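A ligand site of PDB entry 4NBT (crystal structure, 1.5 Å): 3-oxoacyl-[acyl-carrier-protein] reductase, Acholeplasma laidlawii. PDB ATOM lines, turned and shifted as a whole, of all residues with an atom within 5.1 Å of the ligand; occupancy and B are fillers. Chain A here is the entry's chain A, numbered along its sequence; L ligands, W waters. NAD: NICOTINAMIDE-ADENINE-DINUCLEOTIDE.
O of Asp 37 lies within hydrogen-bond range of N of Leu 53, at 3.0 Å. The backbone NH (N) of Gly 39 sits at hydrogen-bond distance from the side-chain carboxylate (OD1) of Asp 37 (3.2 Å). The side-chain carboxylate (OD2) of Asp 37 sits at hydrogen-bond distance from the backbone NH (N) of Gly 14 (3.2 Å). The side-chain hydroxyl (OG) of Ser 132 lies within hydrogen-bond range of the backbone carbonyl oxygen (O) of Lys 150 (2.8 Å). OG1 of Thr 56 is in hydrogen-bond range of OD1 of Asn 54, at 2.8 Å. The backbone NH (N) of Leu 38 is in hydrogen-bond range of the backbone carbonyl oxygen (O) of Leu 53 (3.4 Å). The backbone carbonyl oxygen (O) of Gly 36 lies within hydrogen-bond range of the backbone NH (N) of Gly 13, at 2.8 Å. The backbone carbonyl oxygen of Pro 178 sits at hydrogen-bond distance from the backbone NH of Val 134 (2.9 Å).
Water W6 lies within hydrogen-bond range of O2A of the ligand and OD2 of Asp 184. Water W10 lies within hydrogen-bond range of an oxygen (O1A) of the ligand (2.6 Å) and the side-chain amino group of Lys 16 (2.9 Å). Water W7 lies within hydrogen-bond range of O1A of the ligand (2.6 Å) and O of Gly 83 (2.8 Å). Water W5 lies within hydrogen-bond range of OH of Tyr 146 and OG of Ser 133. Water W11 lies within hydrogen-bond range of O of Ala 82 (2.7 Å), O3D of the ligand (3.2 Å), O of Asn 81 (3.2 Å) and NZ of Lys 150 (3.3 Å).
OD1 of Asp 37 is in hydrogen-bond range of O2B of the ligand (2.6 Å). OH of Tyr 146 is in hydrogen-bond range of O2D of the ligand (2.6 Å). An oxygen (O2N) of the ligand lies within hydrogen-bond range of the backbone NH (N) of Leu 18, at 2.8 Å. The backbone carbonyl oxygen (O) of Asn 81 is in hydrogen-bond range of an oxygen (O3D) of the ligand. An oxygen (O3D) of the ligand sits at hydrogen-bond distance from the side-chain amino group of Lys 150, at 2.9 Å. An oxygen (O1N) of the ligand sits at hydrogen-bond distance from the side-chain hydroxyl (OG1) of Thr 183, 2.9 Å away. N of Ile 181 sits at hydrogen-bond distance from O7N of the ligand (2.9 Å). A nitrogen (N7N) of the ligand lies within hydrogen-bond range of the backbone carbonyl oxygen of Ile 181. A nitrogen (N6A) of the ligand lies within hydrogen-bond range of the side-chain amide oxygen of Asn 54, at 3.0 Å. The backbone NH of Val 55 sits at hydrogen-bond distance from a nitrogen (N1A) of the ligand, 3.1 Å away.
The backbone carbonyl oxygen (O) of Leu 53 lies close to a nitrogen (N1A) of the ligand (3.4 Å). O7N of the ligand sits close to O of Gly 179 (3.4 Å). Merely in contact with the ligand: Ser 132 (3.3 Å), Gly 17 (3.4 Å), Ile 131 (3.4 Å), Gly 13 (3.5 Å), Ser 133 (3.5 Å), Pro 178 (3.5 Å), Lys 16 (3.5 Å), Gly 83 (3.5 Å), Tyr 180 (3.6 Å), Ala 82 (3.6 Å), Leu 38 (3.6 Å), Ile 84 (3.8 Å), Thr 56 (3.96 Å) and Val 104 (3.96 Å). Hydrophobic or aromatic side chains within 4 Å of the ligand: Leu 18, Leu 38, Val 55, Ala 82, Ile 84, Val 104, Ile 131, Tyr 146, Pro 178 and Ile 181. The nearest printed residue that does not touch the ligand is Ala 15 (4.1 Å).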
ATOM      1  N   GLY A  13      13.125  17.170  11.001  1.00  0.00           N
ATOM      2  CA  GLY A  13      13.067  16.679  12.361  1.00  0.00           C
ATOM      3  C   GLY A  13      13.884  17.536  13.321  1.00  0.00           C
ATOM      4  O   GLY A  13      14.517  17.032  14.251  1.00  0.00           O
ATOM      5  N   GLY A  14      13.854  18.851  13.128  1.00  0.00           N
ATOM      6  CA  GLY A  14      14.736  19.746  13.841  1.00  0.00           C
ATOM      7  C   GLY A  14      14.245  20.279  15.189  1.00  0.00           C
ATOM      8  O   GLY A  14      14.910  21.093  15.789  1.00  0.00           O
ATOM      9  N   ALA A  15      13.120  19.783  15.685  1.00  0.00           N
ATOM     10  CA  ALA A  15      12.548  20.347  16.907  1.00  0.00           C
ATOM     11  C   ALA A  15      13.235  19.897  18.197  1.00  0.00           C
ATOM     12  O   ALA A  15      13.148  20.593  19.208  1.00  0.00           O
ATOM     13  CB  ALA A  15      11.069  20.077  16.987  1.00  0.00           C
ATOM     14  N   LYS A  16      13.870  18.732  18.172  1.00  0.00           N
ATOM     15  CA  LYS A  16      14.483  18.155  19.366  1.00  0.00           C
ATOM     16  C   LYS A  16      15.525  17.131  18.922  1.00  0.00           C
ATOM     17  O   LYS A  16      15.736  16.928  17.729  1.00  0.00           O
ATOM     18  CB  LYS A  16      13.417  17.505  20.274  1.00  0.00           C
ATOM     19  CG  LYS A  16      12.733  16.310  19.666  1.00  0.00           C
ATOM     20  CD  LYS A  16      11.718  15.712  20.651  1.00  0.00           C
ATOM     21  CE  LYS A  16      11.194  14.371  20.181  1.00  0.00           C
ATOM     22  NZ  LYS A  16      10.302  13.714  21.178  1.00  0.00           N
ATOM     23  N   GLY A  17      16.163  16.476  19.876  1.00  0.00           N
ATOM     24  CA  GLY A  17      17.059  15.357  19.595  1.00  0.00           C
ATOM     25  C   GLY A  17      18.240  15.740  18.725  1.00  0.00           C
ATOM     26  O   GLY A  17      18.808  16.810  18.861  1.00  0.00           O
ATOM     27  N   LEU A  18      18.636  14.817  17.856  1.00  0.00           N
ATOM     28  CA  LEU A  18      19.800  15.045  16.999  1.00  0.00           C
ATOM     29  C   LEU A  18      19.552  16.243  16.100  1.00  0.00           C
ATOM     30  O   LEU A  18      20.472  16.994  15.829  1.00  0.00           O
ATOM     31  CB  LEU A  18      20.121  13.809  16.157  1.00  0.00           C
ATOM     32  CG  LEU A  18      20.410  12.499  16.917  1.00  0.00           C
ATOM     33  CD1 LEU A  18      20.964  11.454  15.958  1.00  0.00           C
ATOM     34  CD2 LEU A  18      21.398  12.742  18.036  1.00  0.00           C
ATOM     35  N   GLY A  19      18.322  16.391  15.601  1.00  0.00           N
ATOM     36  CA  GLY A  19      18.006  17.509  14.721  1.00  0.00           C
ATOM     37  C   GLY A  19      18.267  18.845  15.380  1.00  0.00           C
ATOM     38  O   GLY A  19      18.838  19.743  14.775  1.00  0.00           O
ATOM     39  N   GLY A  36      12.666  22.129  10.184  1.00  0.00           N
ATOM     40  CA  GLY A  36      11.350  21.641   9.847  1.00  0.00           C
ATOM     41  C   GLY A  36      10.932  20.493  10.754  1.00  0.00           C
ATOM     42  O   GLY A  36      11.713  19.582  10.972  1.00  0.00           O
ATOM     43  N   ASP A  37       9.710  20.526  11.255  1.00  0.00           N
ATOM     44  CA  ASP A  37       9.227  19.483  12.144  1.00  0.00           C
ATOM     45  C   ASP A  37       7.723  19.536  12.247  1.00  0.00           C
ATOM     46  O   ASP A  37       7.099  20.516  11.824  1.00  0.00           O
ATOM     47  CB  ASP A  37       9.872  19.605  13.534  1.00  0.00           C
ATOM     48  CG  ASP A  37      10.022  18.263  14.224  1.00  0.00           C
ATOM     49  OD1 ASP A  37       9.011  17.573  14.433  1.00  0.00           O
ATOM     50  OD2 ASP A  37      11.155  17.892  14.584  1.00  0.00           O
ATOM     51  N   LEU A  38       7.159  18.450  12.754  1.00  0.00           N
ATOM     52  CA  LEU A  38       5.732  18.384  13.059  1.00  0.00           C
ATOM     53  C   LEU A  38       5.440  19.220  14.281  1.00  0.00           C
ATOM     54  O   LEU A  38       4.391  19.844  14.371  1.00  0.00           O
ATOM     55  CB  LEU A  38       5.331  16.934  13.343  1.00  0.00           C
ATOM     56  CG  LEU A  38       5.519  15.929  12.215  1.00  0.00           C
ATOM     57  CD1 LEU A  38       5.290  14.509  12.708  1.00  0.00           C
ATOM     58  CD2 LEU A  38       4.585  16.259  11.076  1.00  0.00           C
ATOM     59  N   GLY A  39       6.351  19.196  15.244  1.00  0.00           N
ATOM     60  CA  GLY A  39       6.145  19.894  16.498  1.00  0.00           C
ATOM     61  C   GLY A  39       6.873  21.217  16.568  1.00  0.00           C
ATOM     62  O   GLY A  39       7.780  21.494  15.776  1.00  0.00           O
ATOM     63  N   LEU A  53       6.811  21.018   8.879  1.00  0.00           N
ATOM     64  CA  LEU A  53       7.194  20.084   7.844  1.00  0.00           C
ATOM     65  C   LEU A  53       6.800  18.692   8.272  1.00  0.00           C
ATOM     66  O   LEU A  53       7.181  18.226   9.337  1.00  0.00           O
ATOM     67  CB  LEU A  53       8.704  20.121   7.614  1.00  0.00           C
ATOM     68  CG  LEU A  53       9.242  19.084   6.637  1.00  0.00           C
ATOM     69  CD1 LEU A  53       8.646  19.276   5.254  1.00  0.00           C
ATOM     70  CD2 LEU A  53      10.764  19.219   6.583  1.00  0.00           C
ATOM     71  N   ASN A  54       5.981  18.052   7.426  1.00  0.00           N
ATOM     72  CA  ASN A  54       5.712  16.618   7.519  1.00  0.00           C
ATOM     73  C   ASN A  54       6.287  15.968   6.285  1.00  0.00           C
ATOM     74  O   ASN A  54       5.763  16.138   5.183  1.00  0.00           O
ATOM     75  CB  ASN A  54       4.196  16.395   7.575  1.00  0.00           C
ATOM     76  CG  ASN A  54       3.834  14.930   7.625  1.00  0.00           C
ATOM     77  OD1 ASN A  54       4.689  14.048   7.577  1.00  0.00           O
ATOM     78  ND2 ASN A  54       2.537  14.672   7.742  1.00  0.00           N
ATOM     79  N   VAL A  55       7.411  15.260   6.446  1.00  0.00           N
ATOM     80  CA  VAL A  55       8.135  14.760   5.295  1.00  0.00           C
ATOM     81  C   VAL A  55       7.357  13.720   4.507  1.00  0.00           C
ATOM     82  O   VAL A  55       7.738  13.432   3.372  1.00  0.00           O
ATOM     83  CB  VAL A  55       9.523  14.171   5.665  1.00  0.00           C
ATOM     84  CG1 VAL A  55      10.424  15.230   6.271  1.00  0.00           C
ATOM     85  CG2 VAL A  55       9.399  12.962   6.592  1.00  0.00           C
ATOM     86  N   THR A  56       6.252  13.226   5.065  1.00  0.00           N
ATOM     87  CA  THR A  56       5.441  12.217   4.389  1.00  0.00           C
ATOM     88  C   THR A  56       4.336  12.813   3.506  1.00  0.00           C
ATOM     89  O   THR A  56       3.724  12.107   2.705  1.00  0.00           O
ATOM     90  CB  THR A  56       4.788  11.195   5.365  1.00  0.00           C
ATOM     91  OG1 THR A  56       3.757  11.816   6.141  1.00  0.00           O
ATOM     92  CG2 THR A  56       5.822  10.537   6.291  1.00  0.00           C
ATOM     93  N   ASN A  81      17.119  14.242   8.651  1.00  0.00           N
ATOM     94  CA  ASN A  81      17.235  13.687  10.004  1.00  0.00           C
ATOM     95  C   ASN A  81      15.926  13.113  10.586  1.00  0.00           C
ATOM     96  O   ASN A  81      15.978  12.215  11.393  1.00  0.00           O
ATOM     97  CB  ASN A  81      17.799  14.781  10.929  1.00  0.00           C
ATOM     98  CG  ASN A  81      17.620  14.477  12.394  1.00  0.00           C
ATOM     99  OD1 ASN A  81      18.414  13.745  13.002  1.00  0.00           O
ATOM    100  ND2 ASN A  81      16.578  15.031  12.982  1.00  0.00           N
ATOM    101  N   ALA A  82      14.767  13.608  10.159  1.00  0.00           N
ATOM    102  CA  ALA A  82      13.498  13.089  10.703  1.00  0.00           C
ATOM    103  C   ALA A  82      13.459  11.575  10.580  1.00  0.00           C
ATOM    104  O   ALA A  82      13.795  11.022   9.537  1.00  0.00           O
ATOM    105  CB  ALA A  82      12.324  13.696   9.995  1.00  0.00           C
ATOM    106  N   GLY A  83      13.056  10.912  11.653  1.00  0.00           N
ATOM    107  CA  GLY A  83      12.969   9.467  11.614  1.00  0.00           C
ATOM    108  C   GLY A  83      12.179   8.960  12.790  1.00  0.00           C
ATOM    109  O   GLY A  83      12.079   9.642  13.825  1.00  0.00           O
ATOM    110  N   ILE A  84      11.607   7.775  12.626  1.00  0.00           N
ATOM    111  CA  ILE A  84      10.837   7.132  13.680  1.00  0.00           C
ATOM    112  C   ILE A  84      11.181   5.645  13.753  1.00  0.00           C
ATOM    113  O   ILE A  84      11.750   5.074  12.821  1.00  0.00           O
ATOM    114  CB  ILE A  84       9.305   7.269  13.435  1.00  0.00           C
ATOM    115  CG1 ILE A  84       8.908   6.614  12.111  1.00  0.00           C
ATOM    116  CG2 ILE A  84       8.867   8.737  13.458  1.00  0.00           C
ATOM    117  CD1 ILE A  84       7.395   6.375  11.968  1.00  0.00           C
ATOM    118  N   VAL A 104       8.277   7.534   6.577  1.00  0.00           N
ATOM    119  CA  VAL A 104       9.091   8.616   7.137  1.00  0.00           C
ATOM    120  C   VAL A 104      10.564   8.483   6.770  1.00  0.00           C
ATOM    121  O   VAL A 104      11.169   9.419   6.250  1.00  0.00           O
ATOM    122  CB  VAL A 104       8.969   8.707   8.676  1.00  0.00           C
ATOM    123  CG1 VAL A 104       9.881   9.777   9.238  1.00  0.00           C
ATOM    124  CG2 VAL A 104       7.518   8.986   9.051  1.00  0.00           C
ATOM    125  N   ASN A 105      11.124   7.301   7.027  1.00  0.00           N
ATOM    126  CA  ASN A 105      12.566   7.160   7.035  1.00  0.00           C
ATOM    127  C   ASN A 105      13.165   6.970   5.665  1.00  0.00           C
ATOM    128  O   ASN A 105      14.367   7.136   5.512  1.00  0.00           O
ATOM    129  CB  ASN A 105      12.982   5.982   7.902  1.00  0.00           C
ATOM    130  CG  ASN A 105      12.649   6.148   9.377  1.00  0.00           C
ATOM    131  OD1 ASN A 105      11.957   7.079   9.804  1.00  0.00           O
ATOM    132  ND2 ASN A 105      13.130   5.214  10.167  1.00  0.00           N
ATOM    133  N   ILE A 131      20.768  10.657   7.559  1.00  0.00           N
ATOM    134  CA  ILE A 131      21.016  10.007   8.838  1.00  0.00           C
ATOM    135  C   ILE A 131      20.606   8.563   8.697  1.00  0.00           C
ATOM    136  O   ILE A 131      19.415   8.250   8.524  1.00  0.00           O
ATOM    137  CB  ILE A 131      20.270  10.694   9.987  1.00  0.00           C
ATOM    138  CG1 ILE A 131      20.604  12.187  10.077  1.00  0.00           C
ATOM    139  CG2 ILE A 131      20.589  10.003  11.312  1.00  0.00           C
ATOM    140  CD1 ILE A 131      22.095  12.511  10.293  1.00  0.00           C
ATOM    141  N   SER A 132      21.599   7.689   8.725  1.00  0.00           N
ATOM    142  CA  SER A 132      21.380   6.247   8.727  1.00  0.00           C
ATOM    143  C   SER A 132      21.315   5.803  10.188  1.00  0.00           C
ATOM    144  O   SER A 132      20.724   6.498  11.017  1.00  0.00           O
ATOM    145  CB  SER A 132      22.480   5.579   7.902  1.00  0.00           C
ATOM    146  OG  SER A 132      22.420   4.153   7.875  1.00  0.00           O
ATOM    147  N   SER A 133      21.934   4.675  10.520  1.00  0.00           N
ATOM    148  CA  SER A 133      22.008   4.171  11.895  1.00  0.00           C
ATOM    149  C   SER A 133      22.902   2.949  11.936  1.00  0.00           C
ATOM    150  O   SER A 133      23.004   2.215  10.953  1.00  0.00           O
ATOM    151  CB  SER A 133      20.627   3.715  12.375  1.00  0.00           C
ATOM    152  OG  SER A 133      20.687   3.027  13.599  1.00  0.00           O
ATOM    153  N   VAL A 134      23.520   2.693  13.081  1.00  0.00           N
ATOM    154  CA  VAL A 134      24.225   1.434  13.315  1.00  0.00           C
ATOM    155  C   VAL A 134      23.304   0.232  12.985  1.00  0.00           C
ATOM    156  O   VAL A 134      23.768  -0.850  12.570  1.00  0.00           O
ATOM    157  CB  VAL A 134      24.760   1.390  14.772  1.00  0.00           C
ATOM    158  CG1 VAL A 134      23.603   1.404  15.774  1.00  0.00           C
ATOM    159  CG2 VAL A 134      25.695   0.194  14.982  1.00  0.00           C
ATOM    160  N   TYR A 146      12.880  -0.640  10.491  1.00  0.00           N
ATOM    161  CA  TYR A 146      13.877   0.404  10.691  1.00  0.00           C
ATOM    162  C   TYR A 146      15.197   0.104   9.992  1.00  0.00           C
ATOM    163  O   TYR A 146      15.776   0.977   9.332  1.00  0.00           O
ATOM    164  CB  TYR A 146      14.110   0.588  12.179  1.00  0.00           C
ATOM    165  CG  TYR A 146      14.965   1.761  12.576  1.00  0.00           C
ATOM    166  CD1 TYR A 146      14.476   3.056  12.500  1.00  0.00           C
ATOM    167  CD2 TYR A 146      16.241   1.585  13.048  1.00  0.00           C
ATOM    168  CE1 TYR A 146      15.248   4.143  12.881  1.00  0.00           C
ATOM    169  CE2 TYR A 146      17.016   2.653  13.419  1.00  0.00           C
ATOM    170  CZ  TYR A 146      16.525   3.924  13.348  1.00  0.00           C
ATOM    171  OH  TYR A 146      17.335   4.965  13.752  1.00  0.00           O
ATOM    172  N   LYS A 150      17.198   2.279   7.170  1.00  0.00           N
ATOM    173  CA  LYS A 150      18.489   2.916   7.421  1.00  0.00           C
ATOM    174  C   LYS A 150      19.566   2.327   6.537  1.00  0.00           C
ATOM    175  O   LYS A 150      20.534   3.021   6.199  1.00  0.00           O
ATOM    176  CB  LYS A 150      18.833   2.855   8.906  1.00  0.00           C
ATOM    177  CG  LYS A 150      17.849   3.674   9.799  1.00  0.00           C
ATOM    178  CD  LYS A 150      17.741   5.118   9.347  1.00  0.00           C
ATOM    179  CE  LYS A 150      17.132   6.016  10.422  1.00  0.00           C
ATOM    180  NZ  LYS A 150      17.170   7.425   9.965  1.00  0.00           N
ATOM    181  N   PRO A 178      24.644   7.013  13.163  1.00  0.00           N
ATOM    182  CA  PRO A 178      24.918   7.092  14.592  1.00  0.00           C
ATOM    183  C   PRO A 178      24.774   5.742  15.274  1.00  0.00           C
ATOM    184  O   PRO A 178      23.964   4.905  14.844  1.00  0.00           O
ATOM    185  CB  PRO A 178      23.817   8.040  15.125  1.00  0.00           C
ATOM    186  CG  PRO A 178      23.300   8.781  13.904  1.00  0.00           C
ATOM    187  CD  PRO A 178      23.437   7.775  12.786  1.00  0.00           C
ATOM    188  N   GLY A 179      25.543   5.539  16.338  1.00  0.00           N
ATOM    189  CA  GLY A 179      25.295   4.491  17.302  1.00  0.00           C
ATOM    190  C   GLY A 179      24.172   4.929  18.219  1.00  0.00           C
ATOM    191  O   GLY A 179      23.311   5.713  17.805  1.00  0.00           O
ATOM    192  N   TYR A 180      24.186   4.485  19.462  1.00  0.00           N
ATOM    193  CA  TYR A 180      23.130   4.816  20.410  1.00  0.00           C
ATOM    194  C   TYR A 180      23.476   6.107  21.119  1.00  0.00           C
ATOM    195  O   TYR A 180      24.522   6.215  21.782  1.00  0.00           O
ATOM    196  CB  TYR A 180      22.932   3.658  21.359  1.00  0.00           C
ATOM    197  CG  TYR A 180      22.228   2.498  20.686  1.00  0.00           C
ATOM    198  CD1 TYR A 180      22.951   1.582  19.963  1.00  0.00           C
ATOM    199  CD2 TYR A 180      20.849   2.372  20.727  1.00  0.00           C
ATOM    200  CE1 TYR A 180      22.339   0.528  19.330  1.00  0.00           C
ATOM    201  CE2 TYR A 180      20.224   1.317  20.081  1.00  0.00           C
ATOM    202  CZ  TYR A 180      20.989   0.385  19.384  1.00  0.00           C
ATOM    203  OH  TYR A 180      20.386  -0.672  18.741  1.00  0.00           O
ATOM    204  N   ILE A 181      22.611   7.097  20.913  1.00  0.00           N
ATOM    205  CA  ILE A 181      22.867   8.461  21.330  1.00  0.00           C
ATOM    206  C   ILE A 181      21.781   8.865  22.286  1.00  0.00           C
ATOM    207  O   ILE A 181      20.594   8.588  22.074  1.00  0.00           O
ATOM    208  CB  ILE A 181      22.845   9.442  20.141  1.00  0.00           C
ATOM    209  CG1 ILE A 181      23.671   8.936  18.963  1.00  0.00           C
ATOM    210  CG2 ILE A 181      23.376  10.807  20.569  1.00  0.00           C
ATOM    211  CD1 ILE A 181      25.148   8.626  19.269  1.00  0.00           C
ATOM    212  N   THR A 183      19.341  10.717  23.299  1.00  0.00           N
ATOM    213  CA  THR A 183      18.289  11.700  23.028  1.00  0.00           C
ATOM    214  C   THR A 183      17.174  11.368  24.000  1.00  0.00           C
ATOM    215  O   THR A 183      17.311  10.415  24.777  1.00  0.00           O
ATOM    216  CB  THR A 183      17.835  11.697  21.535  1.00  0.00           C
ATOM    217  OG1 THR A 183      17.352  10.405  21.143  1.00  0.00           O
ATOM    218  CG2 THR A 183      18.987  12.098  20.651  1.00  0.00           C
ATOM    219  N   ASP A 184      16.096  12.156  24.007  1.00  0.00           N
ATOM    220  CA  ASP A 184      15.019  11.994  24.993  1.00  0.00           C
ATOM    221  C   ASP A 184      14.583  10.548  25.075  1.00  0.00           C
ATOM    222  O   ASP A 184      14.383   9.988  26.156  1.00  0.00           O
ATOM    223  CB  ASP A 184      13.798  12.847  24.623  1.00  0.00           C
ATOM    224  CG  ASP A 184      14.082  14.328  24.707  1.00  0.00           C
ATOM    225  OD1 ASP A 184      14.739  14.757  25.676  1.00  0.00           O
ATOM    226  OD2 ASP A 184      13.647  15.066  23.789  1.00  0.00           O
ATOM    227  N   ILE A 185      14.462   9.937  23.904  1.00  0.00           N
ATOM    228  CA  ILE A 185      13.923   8.596  23.794  1.00  0.00           C
ATOM    229  C   ILE A 185      14.811   7.541  24.481  1.00  0.00           C
ATOM    230  O   ILE A 185      14.296   6.620  25.130  1.00  0.00           O
ATOM    231  CB  ILE A 185      13.630   8.287  22.296  1.00  0.00           C
ATOM    232  CG1 ILE A 185      12.107   8.298  22.019  1.00  0.00           C
ATOM    233  CG2 ILE A 185      14.250   6.970  21.849  1.00  0.00           C
ATOM    234  CD1 ILE A 185      11.297   7.294  22.840  1.00  0.00           C
ATOM    235  N   LEU A 186      16.133   7.668  24.350  1.00  0.00           N
ATOM    236  CA  LEU A 186      17.071   6.733  24.977  1.00  0.00           C
ATOM    237  C   LEU A 186      17.222   7.032  26.488  1.00  0.00           C
ATOM    238  O   LEU A 186      17.768   6.212  27.236  1.00  0.00           O
ATOM    239  CB  LEU A 186      18.441   6.815  24.286  1.00  0.00           C
ATOM    240  CG  LEU A 186      19.001   5.624  23.496  1.00  0.00           C
ATOM    241  CD1 LEU A 186      20.505   5.656  23.542  1.00  0.00           C
ATOM    242  CD2 LEU A 186      18.548   4.239  23.966  1.00  0.00           C
HETATM  243  PA  NAD L   1      13.710  12.036  18.148  1.00  0.00           P
HETATM  244  O1A NAD L   1      12.478  11.172  18.177  1.00  0.00           O
HETATM  245  O2A NAD L   1      14.197  12.639  19.478  1.00  0.00           O
HETATM  246  O5B NAD L   1      13.488  13.241  17.159  1.00  0.00           O
HETATM  247  C5B NAD L   1      12.926  13.008  15.891  1.00  0.00           C
HETATM  248  C4B NAD L   1      12.301  14.234  15.376  1.00  0.00           C
HETATM  249  O4B NAD L   1      11.875  13.881  14.015  1.00  0.00           O
HETATM  250  C3B NAD L   1      11.111  14.656  16.115  1.00  0.00           C
HETATM  251  O3B NAD L   1      11.216  16.045  16.419  1.00  0.00           O
HETATM  252  C2B NAD L   1      10.016  14.336  15.233  1.00  0.00           C
HETATM  253  O2B NAD L   1       8.852  15.182  15.453  1.00  0.00           O
HETATM  254  C1B NAD L   1      10.553  14.446  13.876  1.00  0.00           C
HETATM  255  N9A NAD L   1       9.712  13.769  12.957  1.00  0.00           N
HETATM  256  C8A NAD L   1       9.139  12.527  13.069  1.00  0.00           C
HETATM  257  N7A NAD L   1       8.352  12.281  12.011  1.00  0.00           N
HETATM  258  C5A NAD L   1       8.357  13.375  11.187  1.00  0.00           C
HETATM  259  C6A NAD L   1       7.764  13.729   9.984  1.00  0.00           C
HETATM  260  N6A NAD L   1       6.846  12.877   9.312  1.00  0.00           N
HETATM  261  N1A NAD L   1       8.033  14.946   9.442  1.00  0.00           N
HETATM  262  C2A NAD L   1       8.862  15.810  10.039  1.00  0.00           C
HETATM  263  N3A NAD L   1       9.464  15.515  11.211  1.00  0.00           N
HETATM  264  C4A NAD L   1       9.238  14.312  11.782  1.00  0.00           C
HETATM  265  O3  NAD L   1      14.832  11.095  17.561  1.00  0.00           O
HETATM  266  PN  NAD L   1      16.395  11.316  17.336  1.00  0.00           P
HETATM  267  O1N NAD L   1      17.090  10.313  18.286  1.00  0.00           O
HETATM  268  O2N NAD L   1      16.870  12.737  17.447  1.00  0.00           O
HETATM  269  O5D NAD L   1      16.565  10.812  15.816  1.00  0.00           O
HETATM  270  C5D NAD L   1      17.058  11.645  14.747  1.00  0.00           C
HETATM  271  C4D NAD L   1      17.417  10.748  13.634  1.00  0.00           C
HETATM  272  O4D NAD L   1      18.598   9.984  14.110  1.00  0.00           O
HETATM  273  C3D NAD L   1      16.435   9.726  13.245  1.00  0.00           C
HETATM  274  O3D NAD L   1      16.502   9.496  11.830  1.00  0.00           O
HETATM  275  C2D NAD L   1      16.827   8.518  13.910  1.00  0.00           C
HETATM  276  O2D NAD L   1      16.318   7.352  13.263  1.00  0.00           O
HETATM  277  C1D NAD L   1      18.268   8.585  13.827  1.00  0.00           C
HETATM  278  N1N NAD L   1      19.024   7.828  14.738  1.00  0.00           N
HETATM  279  C2N NAD L   1      18.981   8.058  16.104  1.00  0.00           C
HETATM  280  C3N NAD L   1      19.780   7.294  16.947  1.00  0.00           C
HETATM  281  C7N NAD L   1      19.755   7.493  18.436  1.00  0.00           C
HETATM  282  O7N NAD L   1      20.321   6.652  19.200  1.00  0.00           O
HETATM  283  N7N NAD L   1      19.151   8.717  19.014  1.00  0.00           N
HETATM  284  C4N NAD L   1      20.637   6.355  16.420  1.00  0.00           C
HETATM  285  C5N NAD L   1      20.707   6.176  15.055  1.00  0.00           C
HETATM  286  C6N NAD L   1      19.914   6.925  14.223  1.00  0.00           C
HETATM  287  O   HOH W   1       6.501  14.324  16.381  1.00  0.00           O
HETATM  288  O   HOH W   2      13.919   7.129  15.521  1.00  0.00           O
HETATM  289  O   HOH W   3      15.784   7.736  18.981  1.00  0.00           O
HETATM  290  O   HOH W   4       4.794  10.798  10.254  1.00  0.00           O
HETATM  291  O   HOH W   5      18.999   3.934  15.362  1.00  0.00           O
HETATM  292  O   HOH W   6      14.833  13.609  21.723  1.00  0.00           O
HETATM  293  O   HOH W   7      11.239   9.578  16.497  1.00  0.00           O
HETATM  294  O   HOH W   8      15.962  14.756  15.882  1.00  0.00           O
HETATM  295  O   HOH W   9       6.014  10.762  12.628  1.00  0.00           O
HETATM  296  O   HOH W  10      10.280  11.274  19.600  1.00  0.00           O
HETATM  297  O   HOH W  11      16.298  10.394   8.736  1.00  0.00           O
HETATM  298  O   HOH W  12       8.876  11.238  16.353  1.00  0.00           O
